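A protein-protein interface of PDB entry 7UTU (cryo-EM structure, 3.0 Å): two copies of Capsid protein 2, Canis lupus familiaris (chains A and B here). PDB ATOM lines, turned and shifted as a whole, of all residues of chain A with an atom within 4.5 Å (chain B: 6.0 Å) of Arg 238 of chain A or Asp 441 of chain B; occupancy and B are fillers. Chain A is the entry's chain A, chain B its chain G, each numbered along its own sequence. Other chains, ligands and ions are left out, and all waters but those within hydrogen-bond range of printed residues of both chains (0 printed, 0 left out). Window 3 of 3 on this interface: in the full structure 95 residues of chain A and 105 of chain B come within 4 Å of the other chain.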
ATOM      1  N   SER A  98      -2.604  26.132  15.336  1.00  0.00           N
ATOM      2  CA  SER A  98      -3.896  25.510  15.078  1.00  0.00           C
ATOM      3  C   SER A  98      -3.747  24.091  14.544  1.00  0.00           C
ATOM      4  O   SER A  98      -4.251  23.146  15.154  1.00  0.00           O
ATOM      5  CB  SER A  98      -4.693  26.354  14.083  1.00  0.00           C
ATOM      6  OG  SER A  98      -3.986  26.507  12.870  1.00  0.00           O
ATOM      7  N   PRO A 236      -3.563  16.448   8.480  1.00  0.00           N
ATOM      8  CA  PRO A 236      -3.313  17.410   9.561  1.00  0.00           C
ATOM      9  C   PRO A 236      -4.016  17.030  10.854  1.00  0.00           C
ATOM     10  O   PRO A 236      -5.222  16.779  10.875  1.00  0.00           O
ATOM     11  CB  PRO A 236      -3.861  18.726   8.998  1.00  0.00           C
ATOM     12  CG  PRO A 236      -4.770  18.338   7.924  1.00  0.00           C
ATOM     13  CD  PRO A 236      -4.188  17.116   7.325  1.00  0.00           C
ATOM     14  N   CYS A 237      -3.245  17.000  11.937  1.00  0.00           N
ATOM     15  CA  CYS A 237      -3.797  16.915  13.280  1.00  0.00           C
ATOM     16  C   CYS A 237      -4.085  18.314  13.798  1.00  0.00           C
ATOM     17  O   CYS A 237      -3.238  19.207  13.730  1.00  0.00           O
ATOM     18  CB  CYS A 237      -2.828  16.203  14.218  1.00  0.00           C
ATOM     19  SG  CYS A 237      -3.405  16.093  15.922  1.00  0.00           S
ATOM     20  N   ARG A 238      -5.290  18.496  14.326  1.00  0.00           N
ATOM     21  CA  ARG A 238      -5.812  19.810  14.668  1.00  0.00           C
ATOM     22  C   ARG A 238      -5.719  20.017  16.169  1.00  0.00           C
ATOM     23  O   ARG A 238      -6.148  19.159  16.946  1.00  0.00           O
ATOM     24  CB  ARG A 238      -7.252  19.954  14.195  1.00  0.00           C
ATOM     25  CG  ARG A 238      -7.438  19.458  12.770  1.00  0.00           C
ATOM     26  CD  ARG A 238      -8.661  19.989  12.033  1.00  0.00           C
ATOM     27  NE  ARG A 238      -8.791  21.445  12.075  1.00  0.00           N
ATOM     28  CZ  ARG A 238      -9.192  22.231  11.079  1.00  0.00           C
ATOM     29  NH1 ARG A 238      -9.593  21.748   9.910  1.00  0.00           N
ATOM     30  NH2 ARG A 238      -9.205  23.547  11.265  1.00  0.00           N
ATOM     31  N   LEU A 239      -5.157  21.158  16.568  1.00  0.00           N
ATOM     32  CA  LEU A 239      -4.957  21.509  17.967  1.00  0.00           C
ATOM     33  C   LEU A 239      -6.085  22.373  18.512  1.00  0.00           C
ATOM     34  O   LEU A 239      -5.851  23.223  19.381  1.00  0.00           O
ATOM     35  CB  LEU A 239      -3.612  22.214  18.143  1.00  0.00           C
ATOM     36  CG  LEU A 239      -2.368  21.442  17.712  1.00  0.00           C
ATOM     37  CD1 LEU A 239      -1.189  22.387  17.593  1.00  0.00           C
ATOM     38  CD2 LEU A 239      -2.056  20.333  18.698  1.00  0.00           C
ATOM     39  N   THR A 240      -7.300  22.178  18.011  1.00  0.00           N
ATOM     40  CA  THR A 240      -8.485  22.883  18.462  1.00  0.00           C
ATOM     41  C   THR A 240      -9.610  21.872  18.626  1.00  0.00           C
ATOM     42  O   THR A 240      -9.572  20.784  18.047  1.00  0.00           O
ATOM     43  CB  THR A 240      -8.882  23.975  17.472  1.00  0.00           C
ATOM     44  OG1 THR A 240      -9.160  23.380  16.202  1.00  0.00           O
ATOM     45  CG2 THR A 240      -7.759  24.973  17.305  1.00  0.00           C
ATOM     46  N   LEU A 421     -17.205  12.743  13.812  1.00  0.00           N
ATOM     47  CA  LEU A 421     -16.243  12.589  14.894  1.00  0.00           C
ATOM     48  C   LEU A 421     -15.027  13.453  14.622  1.00  0.00           C
ATOM     49  O   LEU A 421     -14.741  13.817  13.479  1.00  0.00           O
ATOM     50  CB  LEU A 421     -15.775  11.144  15.049  1.00  0.00           C
ATOM     51  CG  LEU A 421     -16.813  10.068  15.325  1.00  0.00           C
ATOM     52  CD1 LEU A 421     -17.109   9.267  14.072  1.00  0.00           C
ATOM     53  CD2 LEU A 421     -16.314   9.158  16.426  1.00  0.00           C
ATOM     54  N   ASN A 422     -14.311  13.763  15.695  1.00  0.00           N
ATOM     55  CA  ASN A 422     -12.980  14.343  15.638  1.00  0.00           C
ATOM     56  C   ASN A 422     -11.939  13.256  15.866  1.00  0.00           C
ATOM     57  O   ASN A 422     -12.200  12.236  16.505  1.00  0.00           O
ATOM     58  CB  ASN A 422     -12.819  15.442  16.687  1.00  0.00           C
ATOM     59  CG  ASN A 422     -13.681  16.647  16.405  1.00  0.00           C
ATOM     60  OD1 ASN A 422     -13.847  17.049  15.255  1.00  0.00           O
ATOM     61  ND2 ASN A 422     -14.234  17.236  17.454  1.00  0.00           N
ATOM     62  N   ASN A 423     -10.744  13.496  15.342  1.00  0.00           N
ATOM     63  CA  ASN A 423      -9.647  12.573  15.560  1.00  0.00           C
ATOM     64  C   ASN A 423      -9.236  12.602  17.026  1.00  0.00           C
ATOM     65  O   ASN A 423      -9.597  13.509  17.778  1.00  0.00           O
ATOM     66  CB  ASN A 423      -8.467  12.934  14.660  1.00  0.00           C
ATOM     67  CG  ASN A 423      -7.625  11.738  14.285  1.00  0.00           C
ATOM     68  OD1 ASN A 423      -6.454  11.659  14.641  1.00  0.00           O
ATOM     69  ND2 ASN A 423      -8.210  10.807  13.541  1.00  0.00           N
ATOM     70  N   GLN A 541      -5.648  20.115  22.895  1.00  0.00           N
ATOM     71  CA  GLN A 541      -6.599  20.909  22.130  1.00  0.00           C
ATOM     72  C   GLN A 541      -7.217  21.938  23.064  1.00  0.00           C
ATOM     73  O   GLN A 541      -8.040  21.584  23.915  1.00  0.00           O
ATOM     74  CB  GLN A 541      -7.675  20.016  21.518  1.00  0.00           C
ATOM     75  CG  GLN A 541      -7.134  18.993  20.548  1.00  0.00           C
ATOM     76  CD  GLN A 541      -8.204  18.109  19.970  1.00  0.00           C
ATOM     77  OE1 GLN A 541      -9.221  17.850  20.608  1.00  0.00           O
ATOM     78  NE2 GLN A 541      -7.977  17.622  18.760  1.00  0.00           N
ATOM     79  N   ARG A 545     -12.890  25.583  18.207  1.00  0.00           N
ATOM     80  CA  ARG A 545     -13.029  25.586  16.757  1.00  0.00           C
ATOM     81  C   ARG A 545     -14.495  25.735  16.382  1.00  0.00           C
ATOM     82  O   ARG A 545     -15.378  25.201  17.058  1.00  0.00           O
ATOM     83  CB  ARG A 545     -12.468  24.302  16.133  1.00  0.00           C
ATOM     84  CG  ARG A 545     -12.621  24.238  14.617  1.00  0.00           C
ATOM     85  CD  ARG A 545     -11.700  23.230  13.953  1.00  0.00           C
ATOM     86  NE  ARG A 545     -12.208  21.862  14.030  1.00  0.00           N
ATOM     87  CZ  ARG A 545     -11.813  20.920  14.879  1.00  0.00           C
ATOM     88  NH1 ARG A 545     -10.928  21.158  15.835  1.00  0.00           N
ATOM     89  NH2 ARG A 545     -12.332  19.702  14.776  1.00  0.00           N
ATOM     90  N   ASP B 439     -16.626  20.904  10.158  1.00  0.00           N
ATOM     91  CA  ASP B 439     -15.179  21.086  10.169  1.00  0.00           C
ATOM     92  C   ASP B 439     -14.551  20.073  11.135  1.00  0.00           C
ATOM     93  O   ASP B 439     -13.519  20.346  11.755  1.00  0.00           O
ATOM     94  CB  ASP B 439     -14.853  22.537  10.554  1.00  0.00           C
ATOM     95  CG  ASP B 439     -13.390  22.919  10.324  1.00  0.00           C
ATOM     96  OD1 ASP B 439     -12.562  22.048   9.987  1.00  0.00           O
ATOM     97  OD2 ASP B 439     -13.070  24.116  10.487  1.00  0.00           O
ATOM     98  N   THR B 440     -15.182  18.913  11.309  1.00  0.00           N
ATOM     99  CA  THR B 440     -14.595  17.826  12.072  1.00  0.00           C
ATOM    100  C   THR B 440     -13.638  17.030  11.191  1.00  0.00           C
ATOM    101  O   THR B 440     -13.650  17.136   9.963  1.00  0.00           O
ATOM    102  CB  THR B 440     -15.681  16.906  12.626  1.00  0.00           C
ATOM    103  OG1 THR B 440     -16.302  16.191  11.551  1.00  0.00           O
ATOM    104  CG2 THR B 440     -16.736  17.708  13.377  1.00  0.00           C
ATOM    105  N   ASP B 441     -12.794  16.228  11.839  1.00  0.00           N
ATOM    106  CA  ASP B 441     -11.832  15.428  11.091  1.00  0.00           C
ATOM    107  C   ASP B 441     -12.527  14.357  10.259  1.00  0.00           C
ATOM    108  O   ASP B 441     -12.272  14.242   9.057  1.00  0.00           O
ATOM    109  CB  ASP B 441     -10.823  14.800  12.049  1.00  0.00           C
ATOM    110  CG  ASP B 441     -10.050  15.837  12.841  1.00  0.00           C
ATOM    111  OD1 ASP B 441      -9.432  16.725  12.217  1.00  0.00           O
ATOM    112  OD2 ASP B 441     -10.063  15.765  14.088  1.00  0.00           O
ATOM    113  N   LEU B 442     -13.408  13.576  10.879  1.00  0.00           N
ATOM    114  CA  LEU B 442     -14.217  12.573  10.197  1.00  0.00           C
ATOM    115  C   LEU B 442     -15.608  13.146   9.985  1.00  0.00           C
ATOM    116  O   LEU B 442     -16.264  13.561  10.947  1.00  0.00           O
ATOM    117  CB  LEU B 442     -14.313  11.273  10.994  1.00  0.00           C
ATOM    118  CG  LEU B 442     -13.112  10.345  11.219  1.00  0.00           C
ATOM    119  CD1 LEU B 442     -11.829  11.044  11.654  1.00  0.00           C
ATOM    120  CD2 LEU B 442     -13.501   9.282  12.240  1.00  0.00           C
ATOM    121  N   LYS B 443     -16.058  13.148   8.735  1.00  0.00           N
ATOM    122  CA  LYS B 443     -17.208  13.915   8.295  1.00  0.00           C
ATOM    123  C   LYS B 443     -18.372  12.986   7.960  1.00  0.00           C
ATOM    124  O   LYS B 443     -18.146  11.836   7.571  1.00  0.00           O
ATOM    125  CB  LYS B 443     -16.840  14.752   7.065  1.00  0.00           C
ATOM    126  CG  LYS B 443     -15.694  15.722   7.318  1.00  0.00           C
ATOM    127  CD  LYS B 443     -15.315  16.493   6.080  1.00  0.00           C
ATOM    128  CE  LYS B 443     -13.933  17.113   6.217  1.00  0.00           C
ATOM    129  NZ  LYS B 443     -13.864  18.071   7.357  1.00  0.00           N
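The side-chain carboxylate (OD1) of Asp 439 of chain B is in salt-bridge range of the guanidinium group (NH1) of Arg 238 of chain A, at 3.0 Å.
O of Leu 421 of chain A lies close to OG1 of Thr 440 of chain B (3.4 Å).
The backbone NH (N) of Leu 442 of chain B is in hydrogen-bond range of the backbone carbonyl oxygen (O) of Leu 421 of chain A (2.9 Å).
N of Asn 423 of chain A is in hydrogen-bond range of OD2 of Asp 441 of chain B (2.7 Å).
The backbone carbonyl oxygen of Asp 439 of chain B lies within hydrogen-bond range of the guanidinium group of Arg 545 of chain A.
NE2 of Gln 541 of chain A is in hydrogen-bond range of O of Arg 238 of chain A (3.0 Å).
The guanidinium group (NH1) of Arg 545 of chain A lies within hydrogen-bond range of the backbone carbonyl oxygen (O) of Thr 240 of chain A, at 2.6 Å.
OD1 of Asn 422 of chain A is in hydrogen-bond range of NH2 of Arg 545 of chain A (3.1 Å).
The side-chain hydroxyl (OG1) of Thr 440 of chain B sits at hydrogen-bond distance from the backbone carbonyl oxygen (O) of Leu 442 of chain B (2.7 Å).
The backbone carbonyl oxygen of Thr 440 of chain B sits at hydrogen-bond distance from the side-chain amino group of Lys 443 of chain B, at 2.8 Å.
Hydrophobic or aromatic side chains of chain B that line the printed part of chain A: Leu 442.
Among the printed residues, Asp or Glu carboxylates within 4 Å of a Lys or Arg side-chain nitrogen of the other chain: Arg 238 of chain A with Asp 439 of chain B (3.0 Å).
Among the printed residues, merely in contact across the chains: Asn 422 of chain A with Thr 440 of chain B (3.2 Å), Arg 238 of chain A with Asp 441 of chain B (3.4 Å), Leu 421 of chain A with Asp 441 of chain B (3.5 Å), Asn 422 of chain A with Asp 441 of chain B (3.6 Å) and Arg 545 of chain A with Thr 440 of chain B (3.99 Å).
Of chain B, only Asp 439 (3.0 Å) and Asp 441 (3.4 Å) come within 4 Å of Arg 238 of chain A.
Asp 441 of chain B touches just these residues of chain A: Arg 238 (3.4 Å), Leu 421 (3.5 Å), Asn 422 (3.6 Å) and Asn 423 (2.7 Å).
Of the printed residues of chain B, Asn 422 of chain A touches Thr 440 and Asp 441.
Of the printed residues of chain A, Leu 442 of chain B touches Leu 421 (2.9 Å).
Printed residues of chain A within 4 Å of Thr 440 of chain B: Leu 421 (3.3 Å), Asn 422 (3.2 Å) and Arg 545 (3.99 Å).
Of the printed residues of chain B, Leu 421 of chain A touches Thr 440, Asp 441 and Leu 442.
Printed residues of chain A within 4 Å of Asp 439 of chain B: Arg 238 and Arg 545.
Thr 240 of chain A touches none of the printed residues of chain B.
Pro 236 of chain A touches none of the printed residues of chain B.
The nearest residue of chain A that does not touch Asp 441 of chain B is Pro 236 of chain A (4.4 Å).
The nearest printed residue of chain B that does not touch Asn 423 of chain A is Leu 442 of chain B (4.1 Å).
No position is printed for both chains.
Of the 10 pairs that touch across the chains among the printed residues, none has its exchanged pair printed and touching as well.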
